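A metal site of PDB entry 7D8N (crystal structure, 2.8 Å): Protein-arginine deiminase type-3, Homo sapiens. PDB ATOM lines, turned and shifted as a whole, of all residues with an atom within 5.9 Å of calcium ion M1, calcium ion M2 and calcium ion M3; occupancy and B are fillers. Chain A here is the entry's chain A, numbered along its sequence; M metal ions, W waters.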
ATOM      1  N   ASN A 153       8.977 -26.306  -3.718  1.00  0.00           N
ATOM      2  CA  ASN A 153       8.512 -25.021  -4.231  1.00  0.00           C
ATOM      3  C   ASN A 153       9.674 -24.029  -4.275  1.00  0.00           C
ATOM      4  O   ASN A 153       9.763 -23.068  -3.511  1.00  0.00           O
ATOM      5  CB  ASN A 153       7.367 -24.506  -3.362  1.00  0.00           C
ATOM      6  CG  ASN A 153       6.692 -23.292  -3.944  1.00  0.00           C
ATOM      7  OD1 ASN A 153       6.944 -22.919  -5.095  1.00  0.00           O
ATOM      8  ND2 ASN A 153       5.828 -22.659  -3.167  1.00  0.00           N
ATOM      9  N   CYS A 154      10.585 -24.277  -5.224  1.00  0.00           N
ATOM     10  CA  CYS A 154      11.853 -23.567  -5.300  1.00  0.00           C
ATOM     11  C   CYS A 154      11.956 -22.658  -6.528  1.00  0.00           C
ATOM     12  O   CYS A 154      13.064 -22.431  -7.019  1.00  0.00           O
ATOM     13  CB  CYS A 154      13.008 -24.571  -5.294  1.00  0.00           C
ATOM     14  SG  CYS A 154      12.901 -25.806  -6.617  1.00  0.00           S
ATOM     15  N   ASP A 155      10.838 -22.125  -7.032  1.00  0.00           N
ATOM     16  CA  ASP A 155      10.846 -21.513  -8.349  1.00  0.00           C
ATOM     17  C   ASP A 155      10.566 -20.015  -8.394  1.00  0.00           C
ATOM     18  O   ASP A 155      10.680 -19.434  -9.474  1.00  0.00           O
ATOM     19  CB  ASP A 155       9.856 -22.233  -9.283  1.00  0.00           C
ATOM     20  CG  ASP A 155       8.405 -21.965  -8.936  1.00  0.00           C
ATOM     21  OD1 ASP A 155       8.069 -21.956  -7.731  1.00  0.00           O
ATOM     22  OD2 ASP A 155       7.603 -21.776  -9.870  1.00  0.00           O
ATOM     23  N   ARG A 156      10.237 -19.361  -7.287  1.00  0.00           N
ATOM     24  CA  ARG A 156      10.108 -17.894  -7.248  1.00  0.00           C
ATOM     25  C   ARG A 156       9.065 -17.386  -8.254  1.00  0.00           C
ATOM     26  O   ARG A 156       9.380 -16.747  -9.254  1.00  0.00           O
ATOM     27  CB  ARG A 156      11.469 -17.220  -7.483  1.00  0.00           C
ATOM     28  CG  ARG A 156      11.449 -15.708  -7.309  1.00  0.00           C
ATOM     29  CD  ARG A 156      12.508 -15.066  -8.165  1.00  0.00           C
ATOM     30  NE  ARG A 156      13.748 -14.856  -7.431  1.00  0.00           N
ATOM     31  CZ  ARG A 156      14.925 -14.620  -8.005  1.00  0.00           C
ATOM     32  NH1 ARG A 156      15.023 -14.575  -9.319  1.00  0.00           N
ATOM     33  NH2 ARG A 156      16.000 -14.437  -7.259  1.00  0.00           N
ATOM     34  N   ASP A 157       7.810 -17.710  -7.963  1.00  0.00           N
ATOM     35  CA  ASP A 157       6.708 -17.204  -8.774  1.00  0.00           C
ATOM     36  C   ASP A 157       6.379 -15.754  -8.473  1.00  0.00           C
ATOM     37  O   ASP A 157       5.815 -15.061  -9.332  1.00  0.00           O
ATOM     38  CB  ASP A 157       5.438 -18.042  -8.554  1.00  0.00           C
ATOM     39  CG  ASP A 157       5.514 -19.391  -9.235  1.00  0.00           C
ATOM     40  OD1 ASP A 157       6.059 -19.471 -10.360  1.00  0.00           O
ATOM     41  OD2 ASP A 157       5.019 -20.369  -8.644  1.00  0.00           O
ATOM     42  N   GLN A 164      13.306 -17.326  -3.340  1.00  0.00           N
ATOM     43  CA  GLN A 164      12.439 -18.463  -3.622  1.00  0.00           C
ATOM     44  C   GLN A 164      11.155 -18.377  -2.814  1.00  0.00           C
ATOM     45  O   GLN A 164      11.094 -17.764  -1.742  1.00  0.00           O
ATOM     46  CB  GLN A 164      13.173 -19.769  -3.345  1.00  0.00           C
ATOM     47  CG  GLN A 164      14.240 -20.097  -4.384  1.00  0.00           C
ATOM     48  CD  GLN A 164      15.308 -21.034  -3.849  1.00  0.00           C
ATOM     49  OE1 GLN A 164      15.430 -22.178  -4.305  1.00  0.00           O
ATOM     50  NE2 GLN A 164      16.100 -20.556  -2.902  1.00  0.00           N
ATOM     51  N   ASP A 165      10.109 -19.010  -3.335  1.00  0.00           N
ATOM     52  CA  ASP A 165       8.780 -18.884  -2.738  1.00  0.00           C
ATOM     53  C   ASP A 165       8.658 -19.594  -1.406  1.00  0.00           C
ATOM     54  O   ASP A 165       7.803 -19.223  -0.601  1.00  0.00           O
ATOM     55  CB  ASP A 165       7.708 -19.409  -3.703  1.00  0.00           C
ATOM     56  CG  ASP A 165       7.607 -18.577  -4.963  1.00  0.00           C
ATOM     57  OD1 ASP A 165       7.958 -17.379  -4.922  1.00  0.00           O
ATOM     58  OD2 ASP A 165       7.165 -19.119  -6.002  1.00  0.00           O
ATOM     59  N   ASN A 166       9.478 -20.610  -1.151  1.00  0.00           N
ATOM     60  CA  ASN A 166       9.372 -21.405   0.060  1.00  0.00           C
ATOM     61  C   ASN A 166      10.295 -20.922   1.182  1.00  0.00           C
ATOM     62  O   ASN A 166      10.603 -21.693   2.094  1.00  0.00           O
ATOM     63  CB  ASN A 166       9.642 -22.879  -0.248  1.00  0.00           C
ATOM     64  CG  ASN A 166      11.026 -23.126  -0.814  1.00  0.00           C
ATOM     65  OD1 ASN A 166      11.823 -22.199  -0.973  1.00  0.00           O
ATOM     66  ND2 ASN A 166      11.318 -24.379  -1.123  1.00  0.00           N
ATOM     67  N   CYS A 167      10.750 -19.674   1.132  1.00  0.00           N
ATOM     68  CA  CYS A 167      11.617 -19.156   2.179  1.00  0.00           C
ATOM     69  C   CYS A 167      10.852 -18.568   3.356  1.00  0.00           C
ATOM     70  O   CYS A 167      11.347 -18.610   4.477  1.00  0.00           O
ATOM     71  CB  CYS A 167      12.570 -18.105   1.602  1.00  0.00           C
ATOM     72  SG  CYS A 167      13.722 -18.766   0.388  1.00  0.00           S
ATOM     73  N   ASP A 168       9.674 -18.013   3.115  1.00  0.00           N
ATOM     74  CA  ASP A 168       8.872 -17.422   4.170  1.00  0.00           C
ATOM     75  C   ASP A 168       7.822 -18.433   4.644  1.00  0.00           C
ATOM     76  O   ASP A 168       7.856 -19.617   4.304  1.00  0.00           O
ATOM     77  CB  ASP A 168       8.244 -16.115   3.700  1.00  0.00           C
ATOM     78  CG  ASP A 168       7.510 -16.252   2.378  1.00  0.00           C
ATOM     79  OD1 ASP A 168       7.256 -17.402   1.954  1.00  0.00           O
ATOM     80  OD2 ASP A 168       7.186 -15.213   1.779  1.00  0.00           O
ATOM     81  N   GLN A 169       6.882 -17.950   5.454  1.00  0.00           N
ATOM     82  CA  GLN A 169       5.759 -18.746   5.931  1.00  0.00           C
ATOM     83  C   GLN A 169       4.435 -18.145   5.478  1.00  0.00           C
ATOM     84  O   GLN A 169       3.440 -18.168   6.213  1.00  0.00           O
ATOM     85  CB  GLN A 169       5.799 -18.891   7.454  1.00  0.00           C
ATOM     86  CG  GLN A 169       7.023 -19.620   7.970  1.00  0.00           C
ATOM     87  CD  GLN A 169       6.943 -19.896   9.458  1.00  0.00           C
ATOM     88  OE1 GLN A 169       5.892 -19.748  10.075  1.00  0.00           O
ATOM     89  NE2 GLN A 169       8.064 -20.313  10.048  1.00  0.00           N
ATOM     90  N   HIS A 170       4.407 -17.584   4.270  1.00  0.00           N
ATOM     91  CA  HIS A 170       3.210 -16.950   3.741  1.00  0.00           C
ATOM     92  C   HIS A 170       3.078 -17.282   2.266  1.00  0.00           C
ATOM     93  O   HIS A 170       4.045 -17.662   1.602  1.00  0.00           O
ATOM     94  CB  HIS A 170       3.229 -15.429   3.923  1.00  0.00           C
ATOM     95  CG  HIS A 170       3.571 -14.984   5.314  1.00  0.00           C
ATOM     96  ND1 HIS A 170       2.605 -14.769   6.284  1.00  0.00           N
ATOM     97  CD2 HIS A 170       4.754 -14.710   5.897  1.00  0.00           C
ATOM     98  CE1 HIS A 170       3.193 -14.388   7.399  1.00  0.00           C
ATOM     99  NE2 HIS A 170       4.495 -14.336   7.192  1.00  0.00           N
ATOM    100  N   VAL A 171       1.854 -17.155   1.761  1.00  0.00           N
ATOM    101  CA  VAL A 171       1.576 -17.194   0.334  1.00  0.00           C
ATOM    102  C   VAL A 171       1.440 -15.753  -0.142  1.00  0.00           C
ATOM    103  O   VAL A 171       0.595 -14.999   0.361  1.00  0.00           O
ATOM    104  CB  VAL A 171       0.297 -18.005   0.034  1.00  0.00           C
ATOM    105  CG1 VAL A 171      -0.061 -17.904  -1.439  1.00  0.00           C
ATOM    106  CG2 VAL A 171       0.486 -19.458   0.444  1.00  0.00           C
ATOM    107  N   HIS A 172       2.280 -15.362  -1.092  1.00  0.00           N
ATOM    108  CA  HIS A 172       2.311 -13.994  -1.582  1.00  0.00           C
ATOM    109  C   HIS A 172       1.872 -13.853  -3.033  1.00  0.00           C
ATOM    110  O   HIS A 172       1.908 -12.743  -3.567  1.00  0.00           O
ATOM    111  CB  HIS A 172       3.714 -13.403  -1.402  1.00  0.00           C
ATOM    112  CG  HIS A 172       4.052 -13.062   0.014  1.00  0.00           C
ATOM    113  ND1 HIS A 172       3.079 -12.743   0.950  1.00  0.00           N
ATOM    114  CD2 HIS A 172       5.232 -12.987   0.663  1.00  0.00           C
ATOM    115  CE1 HIS A 172       3.660 -12.487   2.115  1.00  0.00           C
ATOM    116  NE2 HIS A 172       4.964 -12.627   1.969  1.00  0.00           N
ATOM    117  N   GLN A 175      -0.485 -17.797  -8.018  1.00  0.00           N
ATOM    118  CA  GLN A 175       0.140 -18.776  -8.901  1.00  0.00           C
ATOM    119  C   GLN A 175       1.057 -19.730  -8.140  1.00  0.00           C
ATOM    120  O   GLN A 175       1.357 -20.811  -8.643  1.00  0.00           O
ATOM    121  CB  GLN A 175       0.906 -18.070 -10.034  1.00  0.00           C
ATOM    122  CG  GLN A 175       1.881 -16.988  -9.584  1.00  0.00           C
ATOM    123  CD  GLN A 175       1.244 -15.616  -9.500  1.00  0.00           C
ATOM    124  OE1 GLN A 175       0.274 -15.413  -8.758  1.00  0.00           O
ATOM    125  NE2 GLN A 175       1.776 -14.672 -10.259  1.00  0.00           N
ATOM    126  N   ASP A 176       1.505 -19.342  -6.945  1.00  0.00           N
ATOM    127  CA  ASP A 176       2.361 -20.216  -6.143  1.00  0.00           C
ATOM    128  C   ASP A 176       1.650 -21.513  -5.773  1.00  0.00           C
ATOM    129  O   ASP A 176       2.294 -22.551  -5.660  1.00  0.00           O
ATOM    130  CB  ASP A 176       2.818 -19.484  -4.886  1.00  0.00           C
ATOM    131  CG  ASP A 176       4.003 -20.163  -4.222  1.00  0.00           C
ATOM    132  OD1 ASP A 176       4.649 -20.999  -4.873  1.00  0.00           O
ATOM    133  OD2 ASP A 176       4.278 -19.857  -3.041  1.00  0.00           O
ATOM    134  N   GLU A 178      -0.088 -23.345  -7.555  1.00  0.00           N
ATOM    135  CA  GLU A 178      -0.014 -24.321  -8.637  1.00  0.00           C
ATOM    136  C   GLU A 178       1.121 -25.317  -8.429  1.00  0.00           C
ATOM    137  O   GLU A 178       1.076 -26.405  -9.026  1.00  0.00           O
ATOM    138  CB  GLU A 178       0.159 -23.605  -9.974  1.00  0.00           C
ATOM    139  CG  GLU A 178      -0.984 -22.654 -10.308  1.00  0.00           C
ATOM    140  CD  GLU A 178      -0.796 -21.974 -11.663  1.00  0.00           C
ATOM    141  OE1 GLU A 178      -1.512 -20.977 -11.911  1.00  0.00           O
ATOM    142  OE2 GLU A 178       0.055 -22.430 -12.454  1.00  0.00           O
ATOM    143  N   ASP A 179       2.130 -24.981  -7.624  1.00  0.00           N
ATOM    144  CA  ASP A 179       3.232 -25.884  -7.318  1.00  0.00           C
ATOM    145  C   ASP A 179       2.927 -26.829  -6.158  1.00  0.00           C
ATOM    146  O   ASP A 179       3.562 -27.884  -6.057  1.00  0.00           O
ATOM    147  CB  ASP A 179       4.501 -25.105  -6.974  1.00  0.00           C
ATOM    148  CG  ASP A 179       4.889 -24.106  -8.045  1.00  0.00           C
ATOM    149  OD1 ASP A 179       4.904 -24.471  -9.233  1.00  0.00           O
ATOM    150  OD2 ASP A 179       5.200 -22.944  -7.689  1.00  0.00           O
ATOM    151  N   PHE A 214      -0.253 -25.106   4.637  1.00  0.00           N
ATOM    152  CA  PHE A 214      -1.147 -23.966   4.850  1.00  0.00           C
ATOM    153  C   PHE A 214      -2.583 -24.457   4.835  1.00  0.00           C
ATOM    154  O   PHE A 214      -2.991 -25.166   3.918  1.00  0.00           O
ATOM    155  CB  PHE A 214      -0.965 -22.905   3.764  1.00  0.00           C
ATOM    156  CG  PHE A 214       0.450 -22.409   3.616  1.00  0.00           C
ATOM    157  CD1 PHE A 214       1.337 -23.066   2.789  1.00  0.00           C
ATOM    158  CD2 PHE A 214       0.874 -21.292   4.310  1.00  0.00           C
ATOM    159  CE1 PHE A 214       2.634 -22.614   2.651  1.00  0.00           C
ATOM    160  CE2 PHE A 214       2.165 -20.831   4.180  1.00  0.00           C
ATOM    161  CZ  PHE A 214       3.050 -21.493   3.344  1.00  0.00           C
ATOM    162  N   GLU A 252       3.815 -27.891   0.665  1.00  0.00           N
ATOM    163  CA  GLU A 252       4.868 -27.183  -0.050  1.00  0.00           C
ATOM    164  C   GLU A 252       6.198 -27.775   0.384  1.00  0.00           C
ATOM    165  O   GLU A 252       6.536 -27.740   1.573  1.00  0.00           O
ATOM    166  CB  GLU A 252       4.795 -25.688   0.264  1.00  0.00           C
ATOM    167  CG  GLU A 252       6.031 -24.898  -0.050  1.00  0.00           C
ATOM    168  CD  GLU A 252       5.946 -23.481   0.489  1.00  0.00           C
ATOM    169  OE1 GLU A 252       5.901 -23.321   1.731  1.00  0.00           O
ATOM    170  OE2 GLU A 252       5.891 -22.538  -0.315  1.00  0.00           O
ATOM    171  N   LYS A 362       2.128 -30.535 -12.054  1.00  0.00           N
ATOM    172  CA  LYS A 362       3.017 -29.485 -12.555  1.00  0.00           C
ATOM    173  C   LYS A 362       4.416 -30.034 -12.800  1.00  0.00           C
ATOM    174  O   LYS A 362       4.912 -30.876 -12.051  1.00  0.00           O
ATOM    175  CB  LYS A 362       3.078 -28.308 -11.576  1.00  0.00           C
ATOM    176  CG  LYS A 362       3.914 -27.148 -12.065  1.00  0.00           C
ATOM    177  CD  LYS A 362       3.408 -25.836 -11.497  1.00  0.00           C
ATOM    178  CE  LYS A 362       2.464 -25.152 -12.463  1.00  0.00           C
ATOM    179  NZ  LYS A 362       3.101 -24.954 -13.793  1.00  0.00           N
ATOM    180  N   LEU A 364       8.362 -28.586 -13.458  1.00  0.00           N
ATOM    181  CA  LEU A 364       9.212 -27.413 -13.310  1.00  0.00           C
ATOM    182  C   LEU A 364      10.619 -27.733 -13.805  1.00  0.00           C
ATOM    183  O   LEU A 364      11.263 -28.640 -13.247  1.00  0.00           O
ATOM    184  CB  LEU A 364       9.270 -26.951 -11.853  1.00  0.00           C
ATOM    185  CG  LEU A 364       7.984 -26.557 -11.137  1.00  0.00           C
ATOM    186  CD1 LEU A 364       8.323 -26.114  -9.732  1.00  0.00           C
ATOM    187  CD2 LEU A 364       7.246 -25.471 -11.889  1.00  0.00           C
ATOM    188  N   PRO A 387       9.598 -17.491 -12.511  1.00  0.00           N
ATOM    189  CA  PRO A 387       8.332 -18.212 -12.393  1.00  0.00           C
ATOM    190  C   PRO A 387       8.344 -19.507 -13.206  1.00  0.00           C
ATOM    191  O   PRO A 387       8.722 -19.522 -14.383  1.00  0.00           O
ATOM    192  CB  PRO A 387       7.302 -17.210 -12.939  1.00  0.00           C
ATOM    193  CG  PRO A 387       8.089 -16.231 -13.737  1.00  0.00           C
ATOM    194  CD  PRO A 387       9.409 -16.129 -13.046  1.00  0.00           C
ATOM    195  N   ASP A 388       7.962 -20.601 -12.543  1.00  0.00           N
ATOM    196  CA  ASP A 388       7.983 -21.935 -13.136  1.00  0.00           C
ATOM    197  C   ASP A 388       9.378 -22.336 -13.618  1.00  0.00           C
ATOM    198  O   ASP A 388       9.542 -23.024 -14.627  1.00  0.00           O
ATOM    199  CB  ASP A 388       6.969 -22.056 -14.276  1.00  0.00           C
ATOM    200  CG  ASP A 388       5.594 -22.465 -13.787  1.00  0.00           C
ATOM    201  OD1 ASP A 388       5.304 -22.256 -12.591  1.00  0.00           O
ATOM    202  OD2 ASP A 388       4.811 -23.011 -14.592  1.00  0.00           O
ATOM    203  N   PHE A 389      10.390 -21.899 -12.882  1.00  0.00           N
ATOM    204  CA  PHE A 389      11.764 -22.331 -13.140  1.00  0.00           C
ATOM    205  C   PHE A 389      12.484 -22.318 -11.791  1.00  0.00           C
ATOM    206  O   PHE A 389      12.779 -21.243 -11.264  1.00  0.00           O
ATOM    207  CB  PHE A 389      12.447 -21.436 -14.159  1.00  0.00           C
ATOM    208  CG  PHE A 389      13.425 -22.163 -15.042  1.00  0.00           C
ATOM    209  CD1 PHE A 389      14.257 -23.152 -14.533  1.00  0.00           C
ATOM    210  CD2 PHE A 389      13.505 -21.872 -16.396  1.00  0.00           C
ATOM    211  CE1 PHE A 389      15.163 -23.815 -15.351  1.00  0.00           C
ATOM    212  CE2 PHE A 389      14.396 -22.541 -17.218  1.00  0.00           C
ATOM    213  CZ  PHE A 389      15.223 -23.517 -16.693  1.00  0.00           C
HETATM  214 CA    CA M   1       5.209 -22.076 -10.190  1.00  0.00          CA
HETATM  215 CA    CA M   2       6.244 -21.203  -6.546  1.00  0.00          CA
HETATM  216 CA    CA M   3       5.855 -18.012   0.120  1.00  0.00          CA
HETATM  217  O   HOH W   1       4.888 -20.270  -0.548  1.00  0.00           O
HETATM  218  O   HOH W   2       5.945 -19.848   1.552  1.00  0.00           O
HETATM  219  O   HOH W   3       2.696 -21.448 -10.593  1.00  0.00           O
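OD2 of Asp 165 lies close to N of Arg 156 (3.3 Å).
The side-chain carboxylate of Glu 252 sits at hydrogen-bond distance from the side-chain amide nitrogen of Asn 153, 2.9 Å away.
O of Asn 153 sits close to ND2 of Asn 166.
OD2 of Asp 168 lies close to NE2 of His 172 (3.4 Å).
The side-chain amino group (NZ) of Lys 362 lies within salt-bridge range of the side-chain carboxylate (OD2) of Asp 388.
Of the 25 residues printed, 4 come within 4 Å of calcium ion M1.
Six residues have an atom within 4 Å of calcium ion M2: Asn 153, Asp 155, Asp 157, Asp 165, Asp 176 and Asp 179.
Calcium ion M1 is bound by the side-chain carboxylate (OD2) of Asp 157 (2.3 Å), the side-chain carboxylate (OD1) of Asp 388 (2.4 Å), the side-chain carboxylate (OD2) of Asp 155 (2.4 Å), the side-chain carboxylate (OD1) of Asp 179 (2.6 Å), water W3 (2.6 Å), the side-chain carboxylate (OD2) of Asp 179 (2.6 Å) and the side-chain carboxylate (OD1) of Asp 157 (2.7 Å).
Calcium ion M1 has seven donor atoms within binding distance.
Calcium ion M2 is bound by OD1 of Asp 155.
Calcium ion M2 is bound by the side-chain carboxylate (OD1) of Asp 176, at 2.3 Å.
The side-chain carboxylate (OD2) of Asp 179 is bound to calcium ion M2, at 2.3 Å.
Calcium ion M2 is bound by the side-chain carboxylate (OD2) of Asp 165 (2.3 Å).
OD1 of Asn 153 binds calcium ion M2, 2.4 Å away.
Calcium ion M2 is bound by OD2 of Asp 157 (2.6 Å).
Calcium ion M2 has six donor atoms within binding distance.
Calcium ion M3 is bound by water W2, O of His 170, OD1 of Asp 168, O of Asp 165 and water W1.
Water W3 lies within hydrogen-bond range of O of Gln 175 (2.4 Å) and OE2 of Glu 178 (3.4 Å).
Water W2 lies within hydrogen-bond range of OE2 of Glu 252 and O of Asp 168.
Water W1 bridges OE2 of Glu 252 (2.5 Å) and OD2 of Asp 176 (2.6 Å).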
